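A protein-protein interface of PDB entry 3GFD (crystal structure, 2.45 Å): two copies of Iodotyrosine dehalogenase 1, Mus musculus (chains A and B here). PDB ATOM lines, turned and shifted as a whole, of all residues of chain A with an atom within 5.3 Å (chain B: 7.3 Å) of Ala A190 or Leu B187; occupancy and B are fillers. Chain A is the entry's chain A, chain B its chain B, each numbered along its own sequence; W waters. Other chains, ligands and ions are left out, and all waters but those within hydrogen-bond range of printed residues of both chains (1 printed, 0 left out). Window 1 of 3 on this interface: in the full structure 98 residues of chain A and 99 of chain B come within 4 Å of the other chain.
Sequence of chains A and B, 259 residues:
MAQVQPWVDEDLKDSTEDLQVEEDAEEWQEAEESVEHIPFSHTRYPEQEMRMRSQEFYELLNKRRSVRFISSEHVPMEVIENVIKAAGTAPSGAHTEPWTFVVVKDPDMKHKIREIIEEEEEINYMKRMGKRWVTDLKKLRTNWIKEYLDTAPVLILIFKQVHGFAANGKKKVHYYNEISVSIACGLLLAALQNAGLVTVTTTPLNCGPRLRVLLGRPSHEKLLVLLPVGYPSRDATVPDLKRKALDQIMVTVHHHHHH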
ATOM      1  N   PHE A  57      13.656  30.605 -27.342  1.00  0.00           N
ATOM      2  CA  PHE A  57      13.796  29.182 -27.400  1.00  0.00           C
ATOM      3  C   PHE A  57      15.290  28.805 -27.270  1.00  0.00           C
ATOM      4  O   PHE A  57      15.662  27.822 -26.613  1.00  0.00           O
ATOM      5  CB  PHE A  57      13.214  28.686 -28.702  1.00  0.00           C
ATOM      6  CG  PHE A  57      13.129  27.227 -28.772  1.00  0.00           C
ATOM      7  CD1 PHE A  57      13.895  26.521 -29.682  1.00  0.00           C
ATOM      8  CD2 PHE A  57      12.349  26.522 -27.862  1.00  0.00           C
ATOM      9  CE1 PHE A  57      13.807  25.131 -29.741  1.00  0.00           C
ATOM     10  CE2 PHE A  57      12.277  25.136 -27.936  1.00  0.00           C
ATOM     11  CZ  PHE A  57      12.984  24.448 -28.874  1.00  0.00           C
ATOM     12  N   LEU A  60      16.115  29.146 -23.595  1.00  0.00           N
ATOM     13  CA  LEU A  60      15.579  28.033 -22.868  1.00  0.00           C
ATOM     14  C   LEU A  60      16.491  26.820 -23.044  1.00  0.00           C
ATOM     15  O   LEU A  60      16.861  26.159 -22.062  1.00  0.00           O
ATOM     16  CB  LEU A  60      14.177  27.712 -23.356  1.00  0.00           C
ATOM     17  CG  LEU A  60      13.547  26.484 -22.696  1.00  0.00           C
ATOM     18  CD1 LEU A  60      12.599  26.947 -21.639  1.00  0.00           C
ATOM     19  CD2 LEU A  60      12.795  25.606 -23.661  1.00  0.00           C
ATOM     20  N   LEU A  61      16.874  26.533 -24.289  1.00  0.00           N
ATOM     21  CA  LEU A  61      17.710  25.385 -24.551  1.00  0.00           C
ATOM     22  C   LEU A  61      19.131  25.535 -24.030  1.00  0.00           C
ATOM     23  O   LEU A  61      19.809  24.527 -23.749  1.00  0.00           O
ATOM     24  CB  LEU A  61      17.759  25.086 -26.039  1.00  0.00           C
ATOM     25  CG  LEU A  61      16.442  24.503 -26.506  1.00  0.00           C
ATOM     26  CD1 LEU A  61      16.566  24.171 -27.952  1.00  0.00           C
ATOM     27  CD2 LEU A  61      16.082  23.265 -25.676  1.00  0.00           C
ATOM     28  N   CYS A 185      15.657  11.680 -30.162  1.00  0.00           N
ATOM     29  CA  CYS A 185      16.351  11.998 -28.910  1.00  0.00           C
ATOM     30  C   CYS A 185      16.484  13.493 -28.676  1.00  0.00           C
ATOM     31  O   CYS A 185      16.235  13.987 -27.559  1.00  0.00           O
ATOM     32  CB  CYS A 185      17.758  11.397 -28.904  1.00  0.00           C
ATOM     33  SG  CYS A 185      18.431  11.349 -27.300  1.00  0.00           S
ATOM     34  N   GLY A 186      16.900  14.200 -29.727  1.00  0.00           N
ATOM     35  CA  GLY A 186      17.014  15.659 -29.698  1.00  0.00           C
ATOM     36  C   GLY A 186      15.669  16.263 -29.292  1.00  0.00           C
ATOM     37  O   GLY A 186      15.621  17.116 -28.414  1.00  0.00           O
ATOM     38  N   LEU A 187      14.564  15.783 -29.872  1.00  0.00           N
ATOM     39  CA  LEU A 187      13.240  16.339 -29.525  1.00  0.00           C
ATOM     40  C   LEU A 187      12.876  16.032 -28.088  1.00  0.00           C
ATOM     41  O   LEU A 187      12.230  16.840 -27.420  1.00  0.00           O
ATOM     42  CB  LEU A 187      12.133  15.864 -30.471  1.00  0.00           C
ATOM     43  CG  LEU A 187      12.313  16.262 -31.963  1.00  0.00           C
ATOM     44  CD1 LEU A 187      11.097  15.886 -32.822  1.00  0.00           C
ATOM     45  CD2 LEU A 187      12.578  17.721 -32.155  1.00  0.00           C
ATOM     46  N   LEU A 188      13.283  14.852 -27.626  1.00  0.00           N
ATOM     47  CA  LEU A 188      12.961  14.403 -26.283  1.00  0.00           C
ATOM     48  C   LEU A 188      13.676  15.329 -25.324  1.00  0.00           C
ATOM     49  O   LEU A 188      13.097  15.764 -24.316  1.00  0.00           O
ATOM     50  CB  LEU A 188      13.467  12.980 -26.083  1.00  0.00           C
ATOM     51  CG  LEU A 188      12.807  12.126 -24.979  1.00  0.00           C
ATOM     52  CD1 LEU A 188      13.074  10.659 -25.160  1.00  0.00           C
ATOM     53  CD2 LEU A 188      13.350  12.475 -23.709  1.00  0.00           C
ATOM     54  N   LEU A 189      14.943  15.635 -25.643  1.00  0.00           N
ATOM     55  CA  LEU A 189      15.796  16.410 -24.746  1.00  0.00           C
ATOM     56  C   LEU A 189      15.258  17.827 -24.629  1.00  0.00           C
ATOM     57  O   LEU A 189      15.220  18.404 -23.536  1.00  0.00           O
ATOM     58  CB  LEU A 189      17.226  16.418 -25.266  1.00  0.00           C
ATOM     59  CG  LEU A 189      18.070  15.160 -24.967  1.00  0.00           C
ATOM     60  CD1 LEU A 189      19.354  15.240 -25.696  1.00  0.00           C
ATOM     61  CD2 LEU A 189      18.333  14.918 -23.454  1.00  0.00           C
ATOM     62  N   ALA A 190      14.830  18.373 -25.768  1.00  0.00           N
ATOM     63  CA  ALA A 190      14.167  19.653 -25.825  1.00  0.00           C
ATOM     64  C   ALA A 190      12.902  19.626 -25.022  1.00  0.00           C
ATOM     65  O   ALA A 190      12.633  20.562 -24.258  1.00  0.00           O
ATOM     66  CB  ALA A 190      13.872  20.057 -27.282  1.00  0.00           C
ATOM     67  N   ALA A 191      12.135  18.556 -25.150  1.00  0.00           N
ATOM     68  CA  ALA A 191      10.848  18.494 -24.468  1.00  0.00           C
ATOM     69  C   ALA A 191      11.082  18.396 -22.948  1.00  0.00           C
ATOM     70  O   ALA A 191      10.307  18.977 -22.116  1.00  0.00           O
ATOM     71  CB  ALA A 191      10.025  17.332 -24.981  1.00  0.00           C
ATOM     72  N   LEU A 192      12.158  17.706 -22.558  1.00  0.00           N
ATOM     73  CA  LEU A 192      12.427  17.591 -21.132  1.00  0.00           C
ATOM     74  C   LEU A 192      12.834  18.945 -20.567  1.00  0.00           C
ATOM     75  O   LEU A 192      12.370  19.313 -19.495  1.00  0.00           O
ATOM     76  CB  LEU A 192      13.498  16.548 -20.844  1.00  0.00           C
ATOM     77  CG  LEU A 192      13.173  15.054 -20.887  1.00  0.00           C
ATOM     78  CD1 LEU A 192      14.511  14.287 -20.960  1.00  0.00           C
ATOM     79  CD2 LEU A 192      12.351  14.607 -19.659  1.00  0.00           C
ATOM     80  N   GLN A 193      13.695  19.683 -21.278  1.00  0.00           N
ATOM     81  CA  GLN A 193      14.121  20.999 -20.823  1.00  0.00           C
ATOM     82  C   GLN A 193      12.912  21.936 -20.753  1.00  0.00           C
ATOM     83  O   GLN A 193      12.721  22.652 -19.761  1.00  0.00           O
ATOM     84  CB  GLN A 193      15.195  21.604 -21.754  1.00  0.00           C
ATOM     85  CG  GLN A 193      15.580  23.071 -21.402  1.00  0.00           C
ATOM     86  CD  GLN A 193      16.240  23.138 -20.032  1.00  0.00           C
ATOM     87  OE1 GLN A 193      16.580  22.096 -19.446  1.00  0.00           O
ATOM     88  NE2 GLN A 193      16.457  24.358 -19.518  1.00  0.00           N
ATOM     89  N   ASN A 194      12.096  21.919 -21.810  1.00  0.00           N
ATOM     90  CA  ASN A 194      10.886  22.727 -21.847  1.00  0.00           C
ATOM     91  C   ASN A 194       9.954  22.415 -20.660  1.00  0.00           C
ATOM     92  O   ASN A 194       9.257  23.299 -20.148  1.00  0.00           O
ATOM     93  CB  ASN A 194      10.126  22.484 -23.137  1.00  0.00           C
ATOM     94  CG  ASN A 194       8.915  23.363 -23.236  1.00  0.00           C
ATOM     95  OD1 ASN A 194       9.063  24.571 -23.355  1.00  0.00           O
ATOM     96  ND2 ASN A 194       7.709  22.781 -23.137  1.00  0.00           N
ATOM     97  N   ALA A 195       9.958  21.161 -20.212  1.00  0.00           N
ATOM     98  CA  ALA A 195       9.066  20.709 -19.113  1.00  0.00           C
ATOM     99  C   ALA A 195       9.659  20.889 -17.718  1.00  0.00           C
ATOM    100  O   ALA A 195       8.982  20.615 -16.736  1.00  0.00           O
ATOM    101  CB  ALA A 195       8.667  19.223 -19.320  1.00  0.00           C
ATOM    102  N   PHE B  57       4.028  21.962 -26.032  1.00  0.00           N
ATOM    103  CA  PHE B  57       5.204  21.718 -26.817  1.00  0.00           C
ATOM    104  C   PHE B  57       4.988  20.497 -27.735  1.00  0.00           C
ATOM    105  O   PHE B  57       5.421  20.512 -28.901  1.00  0.00           O
ATOM    106  CB  PHE B  57       6.413  21.514 -25.908  1.00  0.00           C
ATOM    107  CG  PHE B  57       7.736  21.492 -26.634  1.00  0.00           C
ATOM    108  CD1 PHE B  57       8.545  20.351 -26.604  1.00  0.00           C
ATOM    109  CD2 PHE B  57       8.161  22.588 -27.367  1.00  0.00           C
ATOM    110  CE1 PHE B  57       9.786  20.334 -27.280  1.00  0.00           C
ATOM    111  CE2 PHE B  57       9.389  22.581 -28.033  1.00  0.00           C
ATOM    112  CZ  PHE B  57      10.199  21.473 -27.990  1.00  0.00           C
ATOM    113  N   LEU B  61       5.124  20.620 -31.781  1.00  0.00           N
ATOM    114  CA  LEU B  61       5.987  19.723 -32.561  1.00  0.00           C
ATOM    115  C   LEU B  61       5.176  18.812 -33.482  1.00  0.00           C
ATOM    116  O   LEU B  61       5.570  18.526 -34.602  1.00  0.00           O
ATOM    117  CB  LEU B  61       6.867  18.907 -31.642  1.00  0.00           C
ATOM    118  CG  LEU B  61       7.979  19.746 -30.996  1.00  0.00           C
ATOM    119  CD1 LEU B  61       8.908  18.870 -30.182  1.00  0.00           C
ATOM    120  CD2 LEU B  61       8.796  20.492 -32.067  1.00  0.00           C
ATOM    121  N   VAL B  83      18.168  29.773 -34.649  1.00  0.00           N
ATOM    122  CA  VAL B  83      17.892  28.344 -34.662  1.00  0.00           C
ATOM    123  C   VAL B  83      19.175  27.555 -34.662  1.00  0.00           C
ATOM    124  O   VAL B  83      19.256  26.472 -34.064  1.00  0.00           O
ATOM    125  CB  VAL B  83      16.879  27.884 -35.773  1.00  0.00           C
ATOM    126  CG1 VAL B  83      15.532  28.765 -35.740  1.00  0.00           C
ATOM    127  CG2 VAL B  83      17.509  27.889 -37.149  1.00  0.00           C
ATOM    128  N   LYS B  85      22.123  28.651 -33.245  1.00  0.00           N
ATOM    129  CA  LYS B  85      22.517  28.735 -31.837  1.00  0.00           C
ATOM    130  C   LYS B  85      21.822  27.694 -30.949  1.00  0.00           C
ATOM    131  O   LYS B  85      22.484  27.117 -30.064  1.00  0.00           O
ATOM    132  CB  LYS B  85      22.293  30.118 -31.241  1.00  0.00           C
ATOM    133  CG  LYS B  85      23.100  31.165 -31.944  1.00  0.00           C
ATOM    134  CD  LYS B  85      23.543  32.305 -31.056  1.00  0.00           C
ATOM    135  CE  LYS B  85      22.437  33.235 -30.750  1.00  0.00           C
ATOM    136  NZ  LYS B  85      22.940  34.166 -29.684  1.00  0.00           N
ATOM    137  N   ALA B  86      20.511  27.476 -31.169  1.00  0.00           N
ATOM    138  CA  ALA B  86      19.747  26.485 -30.401  1.00  0.00           C
ATOM    139  C   ALA B  86      20.323  25.113 -30.686  1.00  0.00           C
ATOM    140  O   ALA B  86      20.586  24.369 -29.734  1.00  0.00           O
ATOM    141  CB  ALA B  86      18.253  26.514 -30.753  1.00  0.00           C
ATOM    142  N   ALA B  87      20.542  24.787 -31.970  1.00  0.00           N
ATOM    143  CA  ALA B  87      21.080  23.481 -32.310  1.00  0.00           C
ATOM    144  C   ALA B  87      22.429  23.300 -31.578  1.00  0.00           C
ATOM    145  O   ALA B  87      22.760  22.192 -31.111  1.00  0.00           O
ATOM    146  CB  ALA B  87      21.283  23.333 -33.829  1.00  0.00           C
ATOM    147  N   GLY B  88      23.189  24.391 -31.454  1.00  0.00           N
ATOM    148  CA  GLY B  88      24.514  24.314 -30.825  1.00  0.00           C
ATOM    149  C   GLY B  88      24.503  24.029 -29.327  1.00  0.00           C
ATOM    150  O   GLY B  88      25.576  23.799 -28.760  1.00  0.00           O
ATOM    151  N   THR B  89      23.315  24.083 -28.691  1.00  0.00           N
ATOM    152  CA  THR B  89      23.171  23.791 -27.251  1.00  0.00           C
ATOM    153  C   THR B  89      23.081  22.277 -26.975  1.00  0.00           C
ATOM    154  O   THR B  89      23.028  21.860 -25.829  1.00  0.00           O
ATOM    155  CB  THR B  89      21.940  24.454 -26.616  1.00  0.00           C
ATOM    156  OG1 THR B  89      20.741  23.850 -27.148  1.00  0.00           O
ATOM    157  CG2 THR B  89      21.964  26.016 -26.843  1.00  0.00           C
ATOM    158  N   ALA B  90      23.069  21.468 -28.036  1.00  0.00           N
ATOM    159  CA  ALA B  90      22.876  20.039 -27.912  1.00  0.00           C
ATOM    160  C   ALA B  90      24.009  19.424 -27.057  1.00  0.00           C
ATOM    161  O   ALA B  90      25.125  19.900 -27.072  1.00  0.00           O
ATOM    162  CB  ALA B  90      22.902  19.430 -29.263  1.00  0.00           C
ATOM    163  N   PRO B  91      23.727  18.310 -26.373  1.00  0.00           N
ATOM    164  CA  PRO B  91      24.835  17.590 -25.728  1.00  0.00           C
ATOM    165  C   PRO B  91      25.740  16.992 -26.812  1.00  0.00           C
ATOM    166  O   PRO B  91      25.299  16.830 -27.949  1.00  0.00           O
ATOM    167  CB  PRO B  91      24.128  16.453 -24.983  1.00  0.00           C
ATOM    168  CG  PRO B  91      22.811  16.244 -25.849  1.00  0.00           C
ATOM    169  CD  PRO B  91      22.416  17.662 -26.206  1.00  0.00           C
ATOM    170  N   TRP B  99      30.006  19.719 -34.816  1.00  0.00           N
ATOM    171  CA  TRP B  99      29.075  20.089 -35.853  1.00  0.00           C
ATOM    172  C   TRP B  99      29.447  21.413 -36.534  1.00  0.00           C
ATOM    173  O   TRP B  99      29.921  22.353 -35.890  1.00  0.00           O
ATOM    174  CB  TRP B  99      27.662  20.159 -35.259  1.00  0.00           C
ATOM    175  CG  TRP B  99      27.622  20.804 -33.868  1.00  0.00           C
ATOM    176  CD1 TRP B  99      27.976  22.112 -33.534  1.00  0.00           C
ATOM    177  CD2 TRP B  99      27.186  20.193 -32.644  1.00  0.00           C
ATOM    178  NE1 TRP B  99      27.779  22.335 -32.180  1.00  0.00           N
ATOM    179  CE2 TRP B  99      27.296  21.181 -31.611  1.00  0.00           C
ATOM    180  CE3 TRP B  99      26.715  18.907 -32.307  1.00  0.00           C
ATOM    181  CZ2 TRP B  99      26.955  20.907 -30.263  1.00  0.00           C
ATOM    182  CZ3 TRP B  99      26.354  18.645 -30.983  1.00  0.00           C
ATOM    183  CH2 TRP B  99      26.480  19.645 -29.975  1.00  0.00           C
ATOM    184  N   VAL B 181      25.659  14.927 -33.632  1.00  0.00           N
ATOM    185  CA  VAL B 181      25.234  15.825 -34.623  1.00  0.00           C
ATOM    186  C   VAL B 181      23.774  15.594 -34.959  1.00  0.00           C
ATOM    187  O   VAL B 181      23.033  16.556 -35.152  1.00  0.00           O
ATOM    188  CB  VAL B 181      26.133  15.819 -35.846  1.00  0.00           C
ATOM    189  CG1 VAL B 181      25.617  16.836 -36.841  1.00  0.00           C
ATOM    190  CG2 VAL B 181      27.594  16.162 -35.459  1.00  0.00           C
ATOM    191  N   SER B 182      23.308  14.354 -34.961  1.00  0.00           N
ATOM    192  CA  SER B 182      21.868  14.130 -35.164  1.00  0.00           C
ATOM    193  C   SER B 182      21.008  14.686 -34.042  1.00  0.00           C
ATOM    194  O   SER B 182      19.931  15.274 -34.297  1.00  0.00           O
ATOM    195  CB  SER B 182      21.565  12.664 -35.322  1.00  0.00           C
ATOM    196  OG  SER B 182      22.331  12.162 -36.403  1.00  0.00           O
ATOM    197  N   ILE B 183      21.458  14.563 -32.795  1.00  0.00           N
ATOM    198  CA  ILE B 183      20.713  15.231 -31.706  1.00  0.00           C
ATOM    199  C   ILE B 183      20.631  16.732 -31.996  1.00  0.00           C
ATOM    200  O   ILE B 183      19.538  17.304 -31.950  1.00  0.00           O
ATOM    201  CB  ILE B 183      21.326  14.920 -30.359  1.00  0.00           C
ATOM    202  CG1 ILE B 183      21.005  13.457 -30.008  1.00  0.00           C
ATOM    203  CG2 ILE B 183      20.922  15.956 -29.266  1.00  0.00           C
ATOM    204  CD1 ILE B 183      21.808  12.910 -28.809  1.00  0.00           C
ATOM    205  N   ALA B 184      21.752  17.366 -32.377  1.00  0.00           N
ATOM    206  CA  ALA B 184      21.682  18.808 -32.692  1.00  0.00           C
ATOM    207  C   ALA B 184      20.688  19.105 -33.825  1.00  0.00           C
ATOM    208  O   ALA B 184      19.965  20.110 -33.757  1.00  0.00           O
ATOM    209  CB  ALA B 184      23.060  19.405 -32.994  1.00  0.00           C
ATOM    210  N   CYS B 185      20.641  18.232 -34.835  1.00  0.00           N
ATOM    211  CA  CYS B 185      19.647  18.350 -35.901  1.00  0.00           C
ATOM    212  C   CYS B 185      18.211  18.361 -35.358  1.00  0.00           C
ATOM    213  O   CYS B 185      17.377  19.129 -35.817  1.00  0.00           O
ATOM    214  CB  CYS B 185      19.794  17.203 -36.900  1.00  0.00           C
ATOM    215  SG  CYS B 185      18.696  17.406 -38.291  1.00  0.00           S
ATOM    216  N   GLY B 186      17.932  17.495 -34.393  1.00  0.00           N
ATOM    217  CA  GLY B 186      16.637  17.450 -33.721  1.00  0.00           C
ATOM    218  C   GLY B 186      16.318  18.791 -33.090  1.00  0.00           C
ATOM    219  O   GLY B 186      15.183  19.313 -33.268  1.00  0.00           O
ATOM    220  N   LEU B 187      17.302  19.390 -32.411  1.00  0.00           N
ATOM    221  CA  LEU B 187      17.080  20.678 -31.785  1.00  0.00           C
ATOM    222  C   LEU B 187      16.814  21.728 -32.850  1.00  0.00           C
ATOM    223  O   LEU B 187      15.928  22.602 -32.644  1.00  0.00           O
ATOM    224  CB  LEU B 187      18.259  21.120 -30.897  1.00  0.00           C
ATOM    225  CG  LEU B 187      18.666  20.214 -29.712  1.00  0.00           C
ATOM    226  CD1 LEU B 187      19.596  20.975 -28.740  1.00  0.00           C
ATOM    227  CD2 LEU B 187      17.422  19.780 -28.983  1.00  0.00           C
ATOM    228  N   LEU B 188      17.555  21.652 -33.965  1.00  0.00           N
ATOM    229  CA  LEU B 188      17.379  22.596 -35.060  1.00  0.00           C
ATOM    230  C   LEU B 188      15.952  22.480 -35.602  1.00  0.00           C
ATOM    231  O   LEU B 188      15.291  23.514 -35.848  1.00  0.00           O
ATOM    232  CB  LEU B 188      18.357  22.320 -36.218  1.00  0.00           C
ATOM    233  CG  LEU B 188      18.898  23.475 -37.104  1.00  0.00           C
ATOM    234  CD1 LEU B 188      19.675  22.884 -38.283  1.00  0.00           C
ATOM    235  CD2 LEU B 188      17.861  24.308 -37.644  1.00  0.00           C
ATOM    236  N   LEU B 189      15.482  21.239 -35.800  1.00  0.00           N
ATOM    237  CA  LEU B 189      14.134  21.026 -36.329  1.00  0.00           C
ATOM    238  C   LEU B 189      13.074  21.615 -35.402  1.00  0.00           C
ATOM    239  O   LEU B 189      12.091  22.238 -35.885  1.00  0.00           O
ATOM    240  CB  LEU B 189      13.836  19.541 -36.574  1.00  0.00           C
ATOM    241  CG  LEU B 189      14.615  18.907 -37.754  1.00  0.00           C
ATOM    242  CD1 LEU B 189      14.567  17.383 -37.636  1.00  0.00           C
ATOM    243  CD2 LEU B 189      14.204  19.360 -39.122  1.00  0.00           C
ATOM    244  N   ALA B 190      13.287  21.446 -34.082  1.00  0.00           N
ATOM    245  CA  ALA B 190      12.354  21.969 -33.083  1.00  0.00           C
ATOM    246  C   ALA B 190      12.412  23.479 -33.159  1.00  0.00           C
ATOM    247  O   ALA B 190      11.370  24.122 -33.186  1.00  0.00           O
ATOM    248  CB  ALA B 190      12.698  21.484 -31.652  1.00  0.00           C
ATOM    249  N   ALA B 191      13.617  24.045 -33.245  1.00  0.00           N
ATOM    250  CA  ALA B 191      13.748  25.492 -33.274  1.00  0.00           C
ATOM    251  C   ALA B 191      13.074  26.141 -34.527  1.00  0.00           C
ATOM    252  O   ALA B 191      12.412  27.226 -34.426  1.00  0.00           O
ATOM    253  CB  ALA B 191      15.223  25.903 -33.169  1.00  0.00           C
ATOM    254  N   LEU B 192      13.224  25.465 -35.679  1.00  0.00           N
ATOM    255  CA  LEU B 192      12.580  25.873 -36.917  1.00  0.00           C
ATOM    256  C   LEU B 192      11.071  25.876 -36.750  1.00  0.00           C
ATOM    257  O   LEU B 192      10.427  26.921 -37.005  1.00  0.00           O
ATOM    258  CB  LEU B 192      13.002  25.002 -38.100  1.00  0.00           C
ATOM    259  CG  LEU B 192      14.410  25.247 -38.625  1.00  0.00           C
ATOM    260  CD1 LEU B 192      14.817  24.142 -39.563  1.00  0.00           C
ATOM    261  CD2 LEU B 192      14.537  26.575 -39.336  1.00  0.00           C
ATOM    262  N   GLN B 193      10.504  24.763 -36.283  1.00  0.00           N
ATOM    263  CA  GLN B 193       9.056  24.712 -35.980  1.00  0.00           C
ATOM    264  C   GLN B 193       8.584  25.831 -34.991  1.00  0.00           C
ATOM    265  O   GLN B 193       7.558  26.520 -35.218  1.00  0.00           O
ATOM    266  CB  GLN B 193       8.637  23.328 -35.478  1.00  0.00           C
ATOM    267  CG  GLN B 193       7.148  23.150 -35.178  1.00  0.00           C
ATOM    268  CD  GLN B 193       6.284  23.331 -36.431  1.00  0.00           C
ATOM    269  OE1 GLN B 193       6.769  23.229 -37.572  1.00  0.00           O
ATOM    270  NE2 GLN B 193       5.000  23.595 -36.221  1.00  0.00           N
HETATM  271  O   HOH W   1      19.773  22.108 -25.319  1.00  0.00           O
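Ala A190 touches just these residues of chain B: Phe B57 and Leu B187.
Printed residues of chain A within 4 Å of Leu B187: Gly A186 (3.3 Å) and Ala A190 (3.9 Å).
Printed residues of chain A within 4 Å of Ala B191: Phe A57.
Printed residues of chain B within 4 Å of Gly A186: Ile B183 and Leu B187.
Printed residues of chain A within 4 Å of Gly B186: Leu A187.
Of the printed residues of chain B, Asn A194 touches Phe B57 (3.3 Å).
The nearest residue of chain B that does not touch Ala A190 is Ala B190 (4.7 Å).
The nearest printed residue of chain B that does not touch Leu A189 is Leu B187 (5.0 Å).
O of Ala B86 lies within hydrogen-bond range of OG1 of Thr B89 (2.6 Å).
Water W1 bridges OG1 of Thr B89 (2.7 Å) and O of Leu A61 (2.9 Å).
Among the printed residues, merely in contact across the chains: Leu A187 with Gly B186 (3.2 Å), Gly A186 with Leu B187 (3.3 Å), Asn A194 with Phe B57 (3.3 Å), Leu A61 with Thr B89 (3.4 Å), Ala A191 with Phe B57 (3.5 Å), Phe A57 with Ala B191 (3.6 Å), Leu A189 with Pro B91 (3.6 Å), Gly A186 with Ile B183 (3.8 Å), Leu A187 with Ala B190 (3.8 Å), Phe A57 with Phe B57 (3.9 Å), Ala A190 with Phe B57 (3.9 Å), Ala A190 with Leu B187 (3.9 Å) and Leu A189 with Ile B183 (3.96 Å).
Phe B57 touches its own counterpart, Phe A57.
Phe A57 touches Ala B191, and with the chains exchanged Ala A191 touches Phe B57.
Gly A186 touches Leu B187, and with the chains exchanged Leu A187 touches Gly B186.
Ala A190 touches Phe B57, but with the chains exchanged Phe A57 does not touch Ala B190 (4.04 Å).
Of the 13 pairs that touch across the chains among the printed residues, 7 have their exchanged pair printed and touching as well.
Of the 14 printed residues of chain A, 8 touch a printed residue of chain B.
Hydrophobic or aromatic side chains of chain A within 4 Å of the printed part of chain B: Phe A57, Leu A61, Leu A187, Leu A189, Ala A190 and Ala A191.
Of the 24 printed residues of chain B, 8 touch a printed residue of chain A.
Printed residues of chain B that touch a printed residue of chain A: Phe B57, Thr B89, Pro B91, Ile B183, Gly B186, Leu B187, Ala B190 and Ala B191.
Hydrophobic or aromatic side chains of chain B within 4 Å of the printed part of chain A: Phe B57, Pro B91, Ile B183, Leu B187, Ala B190 and Ala B191.
Among the printed residues, 13 pairs touch across the chains.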
